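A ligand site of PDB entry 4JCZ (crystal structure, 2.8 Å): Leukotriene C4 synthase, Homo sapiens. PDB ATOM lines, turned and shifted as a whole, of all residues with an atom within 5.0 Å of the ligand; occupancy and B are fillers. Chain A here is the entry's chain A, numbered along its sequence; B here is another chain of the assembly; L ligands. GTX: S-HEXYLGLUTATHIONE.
OE2 of Glu 64 sits at hydrogen-bond distance from NE2 of Gln 59 of chain B (3.0 Å). The side-chain hydroxyl (OH) of Tyr 99 sits at hydrogen-bond distance from the side-chain amide nitrogen (ND2) of Asn 61, at 2.9 Å. The side-chain hydroxyl (OG) of Ser 29 of chain B sits at hydrogen-bond distance from the side-chain hydroxyl (OH) of Tyr 65 (3.0 Å).
Residues that only touch the ligand: Tyr 65, Ile 33 of chain B, Tyr 56 of chain B, Trp 122, Leu 114, Val 32 of chain B, Ser 29 of chain B, Ala 26 of chain B, Leu 121 and Leu 30 of chain B. Hydrophobic or aromatic side chains within 4 Å of the ligand: Tyr 65, Tyr 99, Leu 114, Leu 121, Trp 122, Ala 26 of chain B, Leu 30 of chain B, Val 32 of chain B, Ile 33 of chain B and Tyr 56 of chain B. 16 residues have an atom within 4 Å of the ligand: Asn 61, Glu 64, Tyr 65, Tyr 99, Arg 110, Leu 114, Leu 121, Trp 122, Ala 26 of chain B, Ser 29 of chain B, Leu 30 of chain B, Val 32 of chain B, Ile 33 of chain B, Arg 36 of chain B, Tyr 56 of chain B and Gln 59 of chain B. The nearest printed residue that does not touch the ligand is Ala 118 (4.2 Å).
The guanidinium group of Arg 36 of chain B lies within salt-bridge range of an oxygen (O12) of the ligand, at 2.7 Å. The side-chain amide oxygen (OE1) of Gln 59 of chain B lies close to a nitrogen (N1) of the ligand (3.3 Å). O31 of the ligand sits at hydrogen-bond distance from OH of Tyr 99. A nitrogen (N1) of the ligand is in salt-bridge range of the side-chain carboxylate (OE1) of Glu 64. The side-chain amide nitrogen (ND2) of Asn 61 lies close to an oxygen (O31) of the ligand, 3.4 Å away. An oxygen (O32) of the ligand is in salt-bridge range of the guanidinium group of Arg 110.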
ATOM      1  N   ASN A  61      -1.895  -3.909   3.683  1.00  0.00           N
ATOM      2  CA  ASN A  61      -1.230  -2.864   2.883  1.00  0.00           C
ATOM      3  C   ASN A  61      -1.181  -3.265   1.417  1.00  0.00           C
ATOM      4  O   ASN A  61      -1.380  -2.438   0.499  1.00  0.00           O
ATOM      5  CB  ASN A  61       0.190  -2.560   3.389  1.00  0.00           C
ATOM      6  CG  ASN A  61       0.185  -1.824   4.708  1.00  0.00           C
ATOM      7  OD1 ASN A  61      -0.850  -1.696   5.370  1.00  0.00           O
ATOM      8  ND2 ASN A  61       1.329  -1.295   5.082  1.00  0.00           N
ATOM      9  N   GLU A  64      -4.582  -2.691  -0.034  1.00  0.00           N
ATOM     10  CA  GLU A  64      -4.854  -1.281  -0.231  1.00  0.00           C
ATOM     11  C   GLU A  64      -4.117  -0.802  -1.509  1.00  0.00           C
ATOM     12  O   GLU A  64      -4.665  -0.005  -2.264  1.00  0.00           O
ATOM     13  CB  GLU A  64      -4.477  -0.520   1.027  1.00  0.00           C
ATOM     14  CG  GLU A  64      -4.135   0.908   0.853  1.00  0.00           C
ATOM     15  CD  GLU A  64      -3.487   1.472   2.104  1.00  0.00           C
ATOM     16  OE1 GLU A  64      -3.620   0.814   3.167  1.00  0.00           O
ATOM     17  OE2 GLU A  64      -2.817   2.539   1.988  1.00  0.00           O
ATOM     18  N   TYR A  65      -2.894  -1.248  -1.760  1.00  0.00           N
ATOM     19  CA  TYR A  65      -2.186  -0.768  -2.948  1.00  0.00           C
ATOM     20  C   TYR A  65      -2.571  -1.491  -4.240  1.00  0.00           C
ATOM     21  O   TYR A  65      -2.232  -1.016  -5.327  1.00  0.00           O
ATOM     22  CB  TYR A  65      -0.669  -0.874  -2.748  1.00  0.00           C
ATOM     23  CG  TYR A  65      -0.161   0.371  -2.090  1.00  0.00           C
ATOM     24  CD1 TYR A  65       0.249   1.420  -2.891  1.00  0.00           C
ATOM     25  CD2 TYR A  65      -0.128   0.535  -0.713  1.00  0.00           C
ATOM     26  CE1 TYR A  65       0.668   2.603  -2.366  1.00  0.00           C
ATOM     27  CE2 TYR A  65       0.329   1.724  -0.162  1.00  0.00           C
ATOM     28  CZ  TYR A  65       0.709   2.758  -1.024  1.00  0.00           C
ATOM     29  OH  TYR A  65       1.177   3.958  -0.572  1.00  0.00           O
ATOM     30  N   LEU A  68      -4.253   0.518  -6.990  1.00  0.00           N
ATOM     31  CA  LEU A  68      -3.446   1.578  -7.553  1.00  0.00           C
ATOM     32  C   LEU A  68      -2.619   0.997  -8.675  1.00  0.00           C
ATOM     33  O   LEU A  68      -2.534   1.542  -9.763  1.00  0.00           O
ATOM     34  CB  LEU A  68      -2.543   2.256  -6.549  1.00  0.00           C
ATOM     35  CG  LEU A  68      -3.346   2.962  -5.463  1.00  0.00           C
ATOM     36  CD1 LEU A  68      -2.335   3.478  -4.493  1.00  0.00           C
ATOM     37  CD2 LEU A  68      -4.325   4.009  -5.960  1.00  0.00           C
ATOM     38  N   ARG A  96       6.360  -6.801  -4.001  1.00  0.00           N
ATOM     39  CA  ARG A  96       5.287  -7.007  -3.029  1.00  0.00           C
ATOM     40  C   ARG A  96       5.324  -8.367  -2.326  1.00  0.00           C
ATOM     41  O   ARG A  96       5.038  -8.460  -1.125  1.00  0.00           O
ATOM     42  CB  ARG A  96       3.905  -6.734  -3.646  1.00  0.00           C
ATOM     43  CG  ARG A  96       3.642  -5.253  -3.820  1.00  0.00           C
ATOM     44  CD  ARG A  96       3.436  -4.689  -2.455  1.00  0.00           C
ATOM     45  NE  ARG A  96       3.144  -3.278  -2.441  1.00  0.00           N
ATOM     46  CZ  ARG A  96       2.774  -2.623  -1.352  1.00  0.00           C
ATOM     47  NH1 ARG A  96       2.556  -3.305  -0.241  1.00  0.00           N
ATOM     48  NH2 ARG A  96       2.539  -1.313  -1.401  1.00  0.00           N
ATOM     49  N   TYR A  99       8.053  -7.895   0.132  1.00  0.00           N
ATOM     50  CA  TYR A  99       7.517  -7.074   1.201  1.00  0.00           C
ATOM     51  C   TYR A  99       6.718  -7.949   2.204  1.00  0.00           C
ATOM     52  O   TYR A  99       6.965  -7.892   3.406  1.00  0.00           O
ATOM     53  CB  TYR A  99       6.644  -5.957   0.620  1.00  0.00           C
ATOM     54  CG  TYR A  99       5.793  -5.220   1.612  1.00  0.00           C
ATOM     55  CD1 TYR A  99       6.294  -4.097   2.264  1.00  0.00           C
ATOM     56  CD2 TYR A  99       4.495  -5.626   1.912  1.00  0.00           C
ATOM     57  CE1 TYR A  99       5.532  -3.403   3.184  1.00  0.00           C
ATOM     58  CE2 TYR A  99       3.723  -4.922   2.833  1.00  0.00           C
ATOM     59  CZ  TYR A  99       4.261  -3.822   3.470  1.00  0.00           C
ATOM     60  OH  TYR A  99       3.501  -3.100   4.338  1.00  0.00           O
ATOM     61  N   ARG A 110      10.615  -5.695   6.001  1.00  0.00           N
ATOM     62  CA  ARG A 110       9.613  -5.330   5.022  1.00  0.00           C
ATOM     63  C   ARG A 110      10.125  -4.114   4.202  1.00  0.00           C
ATOM     64  O   ARG A 110       9.691  -3.890   3.081  1.00  0.00           O
ATOM     65  CB  ARG A 110       8.269  -4.982   5.672  1.00  0.00           C
ATOM     66  CG  ARG A 110       8.107  -3.501   5.988  1.00  0.00           C
ATOM     67  CD  ARG A 110       6.916  -3.220   6.879  1.00  0.00           C
ATOM     68  NE  ARG A 110       6.647  -1.783   6.990  1.00  0.00           N
ATOM     69  CZ  ARG A 110       7.353  -0.950   7.738  1.00  0.00           C
ATOM     70  NH1 ARG A 110       7.034   0.352   7.812  1.00  0.00           N
ATOM     71  NH2 ARG A 110       8.381  -1.397   8.442  1.00  0.00           N
ATOM     72  N   LEU A 114       9.571  -2.950   0.158  1.00  0.00           N
ATOM     73  CA  LEU A 114       8.672  -1.805   0.083  1.00  0.00           C
ATOM     74  C   LEU A 114       9.149  -0.700  -0.857  1.00  0.00           C
ATOM     75  O   LEU A 114       8.381  -0.188  -1.681  1.00  0.00           O
ATOM     76  CB  LEU A 114       8.356  -1.224   1.457  1.00  0.00           C
ATOM     77  CG  LEU A 114       7.437  -0.002   1.431  1.00  0.00           C
ATOM     78  CD1 LEU A 114       6.072  -0.391   0.810  1.00  0.00           C
ATOM     79  CD2 LEU A 114       7.311   0.697   2.760  1.00  0.00           C
ATOM     80  N   ALA A 118       7.611   0.629  -4.468  1.00  0.00           N
ATOM     81  CA  ALA A 118       7.244   2.016  -4.738  1.00  0.00           C
ATOM     82  C   ALA A 118       7.936   2.578  -5.982  1.00  0.00           C
ATOM     83  O   ALA A 118       7.343   3.356  -6.722  1.00  0.00           O
ATOM     84  CB  ALA A 118       7.514   2.908  -3.546  1.00  0.00           C
ATOM     85  N   LEU A 121       6.088   1.196  -8.931  1.00  0.00           N
ATOM     86  CA  LEU A 121       4.794   1.827  -9.014  1.00  0.00           C
ATOM     87  C   LEU A 121       4.872   3.265  -9.542  1.00  0.00           C
ATOM     88  O   LEU A 121       4.003   3.691 -10.306  1.00  0.00           O
ATOM     89  CB  LEU A 121       4.066   1.752  -7.678  1.00  0.00           C
ATOM     90  CG  LEU A 121       2.619   2.207  -7.674  1.00  0.00           C
ATOM     91  CD1 LEU A 121       1.843   1.378  -8.706  1.00  0.00           C
ATOM     92  CD2 LEU A 121       2.038   1.978  -6.327  1.00  0.00           C
ATOM     93  N   TRP A 122       5.850   4.056  -9.089  1.00  0.00           N
ATOM     94  CA  TRP A 122       5.991   5.414  -9.616  1.00  0.00           C
ATOM     95  C   TRP A 122       6.438   5.404 -11.068  1.00  0.00           C
ATOM     96  O   TRP A 122       6.106   6.291 -11.830  1.00  0.00           O
ATOM     97  CB  TRP A 122       6.971   6.268  -8.804  1.00  0.00           C
ATOM     98  CG  TRP A 122       6.531   6.652  -7.443  1.00  0.00           C
ATOM     99  CD1 TRP A 122       6.823   6.025  -6.254  1.00  0.00           C
ATOM    100  CD2 TRP A 122       5.621   7.703  -7.118  1.00  0.00           C
ATOM    101  NE1 TRP A 122       6.200   6.670  -5.207  1.00  0.00           N
ATOM    102  CE2 TRP A 122       5.448   7.703  -5.718  1.00  0.00           C
ATOM    103  CE3 TRP A 122       4.929   8.670  -7.883  1.00  0.00           C
ATOM    104  CZ2 TRP A 122       4.619   8.611  -5.058  1.00  0.00           C
ATOM    105  CZ3 TRP A 122       4.108   9.576  -7.229  1.00  0.00           C
ATOM    106  CH2 TRP A 122       3.955   9.535  -5.826  1.00  0.00           C
ATOM    107  N   VAL A 125       3.403   5.066 -12.937  1.00  0.00           N
ATOM    108  CA  VAL A 125       2.773   6.370 -12.930  1.00  0.00           C
ATOM    109  C   VAL A 125       3.368   7.318 -13.956  1.00  0.00           C
ATOM    110  O   VAL A 125       2.657   8.066 -14.622  1.00  0.00           O
ATOM    111  CB  VAL A 125       2.790   6.995 -11.509  1.00  0.00           C
ATOM    112  CG1 VAL A 125       2.401   8.470 -11.533  1.00  0.00           C
ATOM    113  CG2 VAL A 125       1.853   6.221 -10.615  1.00  0.00           C
ATOM    114  N   VAL B  22      -5.256   8.012  -8.702  1.00  0.00           N
ATOM    115  CA  VAL B  22      -4.106   7.275  -8.183  1.00  0.00           C
ATOM    116  C   VAL B  22      -3.173   8.210  -7.448  1.00  0.00           C
ATOM    117  O   VAL B  22      -2.786   7.953  -6.294  1.00  0.00           O
ATOM    118  CB  VAL B  22      -3.339   6.533  -9.301  1.00  0.00           C
ATOM    119  CG1 VAL B  22      -2.023   5.998  -8.784  1.00  0.00           C
ATOM    120  CG2 VAL B  22      -4.192   5.394  -9.859  1.00  0.00           C
ATOM    121  N   ALA B  26      -2.032   8.277  -3.442  1.00  0.00           N
ATOM    122  CA  ALA B  26      -0.621   8.262  -3.094  1.00  0.00           C
ATOM    123  C   ALA B  26      -0.357   9.377  -2.109  1.00  0.00           C
ATOM    124  O   ALA B  26       0.344   9.194  -1.109  1.00  0.00           O
ATOM    125  CB  ALA B  26       0.244   8.445  -4.331  1.00  0.00           C
ATOM    126  N   SER B  29      -1.523   8.428   1.238  1.00  0.00           N
ATOM    127  CA  SER B  29      -0.573   7.497   1.842  1.00  0.00           C
ATOM    128  C   SER B  29       0.647   8.201   2.459  1.00  0.00           C
ATOM    129  O   SER B  29       1.083   7.875   3.579  1.00  0.00           O
ATOM    130  CB  SER B  29      -0.066   6.494   0.803  1.00  0.00           C
ATOM    131  OG  SER B  29      -1.141   5.752   0.254  1.00  0.00           O
ATOM    132  N   LEU B  30       1.191   9.149   1.716  1.00  0.00           N
ATOM    133  CA  LEU B  30       2.333   9.883   2.236  1.00  0.00           C
ATOM    134  C   LEU B  30       1.916  10.716   3.440  1.00  0.00           C
ATOM    135  O   LEU B  30       2.667  10.790   4.413  1.00  0.00           O
ATOM    136  CB  LEU B  30       2.967  10.764   1.148  1.00  0.00           C
ATOM    137  CG  LEU B  30       3.588  10.060  -0.055  1.00  0.00           C
ATOM    138  CD1 LEU B  30       3.946  11.089  -1.113  1.00  0.00           C
ATOM    139  CD2 LEU B  30       4.815   9.232   0.329  1.00  0.00           C
ATOM    140  N   VAL B  32      -0.349   9.825   5.623  1.00  0.00           N
ATOM    141  CA  VAL B  32      -0.388   8.879   6.717  1.00  0.00           C
ATOM    142  C   VAL B  32       1.017   8.600   7.222  1.00  0.00           C
ATOM    143  O   VAL B  32       1.212   8.560   8.422  1.00  0.00           O
ATOM    144  CB  VAL B  32      -1.096   7.567   6.343  1.00  0.00           C
ATOM    145  CG1 VAL B  32      -0.905   6.505   7.423  1.00  0.00           C
ATOM    146  CG2 VAL B  32      -2.560   7.841   6.081  1.00  0.00           C
ATOM    147  N   ILE B  33       1.999   8.415   6.343  1.00  0.00           N
ATOM    148  CA  ILE B  33       3.369   8.172   6.845  1.00  0.00           C
ATOM    149  C   ILE B  33       3.866   9.378   7.671  1.00  0.00           C
ATOM    150  O   ILE B  33       4.509   9.209   8.740  1.00  0.00           O
ATOM    151  CB  ILE B  33       4.349   7.905   5.705  1.00  0.00           C
ATOM    152  CG1 ILE B  33       4.116   6.536   5.105  1.00  0.00           C
ATOM    153  CG2 ILE B  33       5.784   7.901   6.203  1.00  0.00           C
ATOM    154  CD1 ILE B  33       4.880   6.401   3.851  1.00  0.00           C
ATOM    155  N   ARG B  36       2.356   9.251  11.004  1.00  0.00           N
ATOM    156  CA  ARG B  36       3.093   8.223  11.730  1.00  0.00           C
ATOM    157  C   ARG B  36       4.380   8.768  12.359  1.00  0.00           C
ATOM    158  O   ARG B  36       4.747   8.399  13.473  1.00  0.00           O
ATOM    159  CB  ARG B  36       3.460   7.022  10.830  1.00  0.00           C
ATOM    160  CG  ARG B  36       2.449   5.890  10.819  1.00  0.00           C
ATOM    161  CD  ARG B  36       2.905   4.713   9.923  1.00  0.00           C
ATOM    162  NE  ARG B  36       1.831   3.743   9.686  1.00  0.00           N
ATOM    163  CZ  ARG B  36       1.325   2.912  10.612  1.00  0.00           C
ATOM    164  NH1 ARG B  36       1.808   2.910  11.839  1.00  0.00           N
ATOM    165  NH2 ARG B  36       0.350   2.079  10.297  1.00  0.00           N
ATOM    166  N   PRO B  43       4.771   1.113  12.644  1.00  0.00           N
ATOM    167  CA  PRO B  43       4.184  -0.162  12.167  1.00  0.00           C
ATOM    168  C   PRO B  43       4.682  -1.463  12.907  1.00  0.00           C
ATOM    169  O   PRO B  43       5.853  -1.512  13.282  1.00  0.00           O
ATOM    170  CB  PRO B  43       4.644  -0.219  10.697  1.00  0.00           C
ATOM    171  CG  PRO B  43       4.863   1.219  10.331  1.00  0.00           C
ATOM    172  CD  PRO B  43       5.424   1.859  11.555  1.00  0.00           C
ATOM    173  N   THR B  46      -2.098   0.599  14.539  1.00  0.00           N
ATOM    174  CA  THR B  46      -2.748   1.613  13.747  1.00  0.00           C
ATOM    175  C   THR B  46      -3.621   2.434  14.706  1.00  0.00           C
ATOM    176  O   THR B  46      -4.548   3.160  14.307  1.00  0.00           O
ATOM    177  CB  THR B  46      -3.597   0.908  12.657  1.00  0.00           C
ATOM    178  OG1 THR B  46      -4.468  -0.058  13.260  1.00  0.00           O
ATOM    179  CG2 THR B  46      -2.687   0.209  11.632  1.00  0.00           C
ATOM    180  N   TYR B  56      -5.346   8.328   9.496  1.00  0.00           N
ATOM    181  CA  TYR B  56      -5.330   6.922   9.147  1.00  0.00           C
ATOM    182  C   TYR B  56      -6.676   6.471   8.611  1.00  0.00           C
ATOM    183  O   TYR B  56      -6.791   5.729   7.621  1.00  0.00           O
ATOM    184  CB  TYR B  56      -4.908   6.050  10.335  1.00  0.00           C
ATOM    185  CG  TYR B  56      -4.992   4.566  10.093  1.00  0.00           C
ATOM    186  CD1 TYR B  56      -4.048   3.921   9.308  1.00  0.00           C
ATOM    187  CD2 TYR B  56      -6.076   3.819  10.576  1.00  0.00           C
ATOM    188  CE1 TYR B  56      -4.138   2.568   9.055  1.00  0.00           C
ATOM    189  CE2 TYR B  56      -6.167   2.474  10.334  1.00  0.00           C
ATOM    190  CZ  TYR B  56      -5.198   1.845   9.559  1.00  0.00           C
ATOM    191  OH  TYR B  56      -5.285   0.485   9.311  1.00  0.00           O
ATOM    192  N   GLN B  59      -7.685   7.962   5.256  1.00  0.00           N
ATOM    193  CA  GLN B  59      -6.982   7.250   4.196  1.00  0.00           C
ATOM    194  C   GLN B  59      -7.611   5.900   3.908  1.00  0.00           C
ATOM    195  O   GLN B  59      -7.798   5.526   2.751  1.00  0.00           O
ATOM    196  CB  GLN B  59      -5.510   7.113   4.539  1.00  0.00           C
ATOM    197  CG  GLN B  59      -4.664   6.305   3.577  1.00  0.00           C
ATOM    198  CD  GLN B  59      -4.620   4.854   4.001  1.00  0.00           C
ATOM    199  OE1 GLN B  59      -4.062   4.543   5.041  1.00  0.00           O
ATOM    200  NE2 GLN B  59      -5.146   3.951   3.184  1.00  0.00           N
HETATM  201  N1  GTX L   1      -2.427   1.763   5.816  1.00  0.00           N
HETATM  202  CA1 GTX L   1      -1.142   2.383   5.646  1.00  0.00           C
HETATM  203  C1  GTX L   1      -0.395   2.484   6.950  1.00  0.00           C
HETATM  204  O11 GTX L   1       0.835   2.743   6.967  1.00  0.00           O
HETATM  205  O12 GTX L   1      -1.022   2.333   8.034  1.00  0.00           O
HETATM  206  CB1 GTX L   1      -1.404   3.736   5.089  1.00  0.00           C
HETATM  207  CG1 GTX L   1      -0.309   4.574   4.547  1.00  0.00           C
HETATM  208  CD1 GTX L   1       0.481   3.901   3.515  1.00  0.00           C
HETATM  209  OE1 GTX L   1       0.045   2.938   2.910  1.00  0.00           O
HETATM  210  N2  GTX L   1       1.777   4.358   3.215  1.00  0.00           N
HETATM  211  CA2 GTX L   1       2.503   3.655   2.193  1.00  0.00           C
HETATM  212  C2  GTX L   1       3.051   2.444   2.889  1.00  0.00           C
HETATM  213  O2  GTX L   1       3.776   1.625   2.302  1.00  0.00           O
HETATM  214  CB2 GTX L   1       3.394   4.689   1.566  1.00  0.00           C
HETATM  215  SG2 GTX L   1       4.812   4.406   0.533  1.00  0.00           S
HETATM  216  C1S GTX L   1       4.686   5.464  -0.859  1.00  0.00           C
HETATM  217  C2S GTX L   1       4.068   4.844  -2.061  1.00  0.00           C
HETATM  218  C3S GTX L   1       3.678   5.754  -3.159  1.00  0.00           C
HETATM  219  C4S GTX L   1       2.731   5.173  -4.147  1.00  0.00           C
HETATM  220  C5S GTX L   1       2.905   5.534  -5.580  1.00  0.00           C
HETATM  221  C6S GTX L   1       1.646   5.676  -6.376  1.00  0.00           C
HETATM  222  N3  GTX L   1       2.636   2.309   4.262  1.00  0.00           N
HETATM  223  CA3 GTX L   1       2.979   1.262   5.173  1.00  0.00           C
HETATM  224  C3  GTX L   1       4.383   0.802   5.166  1.00  0.00           C
HETATM  225  O31 GTX L   1       4.640  -0.396   4.838  1.00  0.00           O
HETATM  226  O32 GTX L   1       5.276   1.652   5.459  1.00  0.00           O
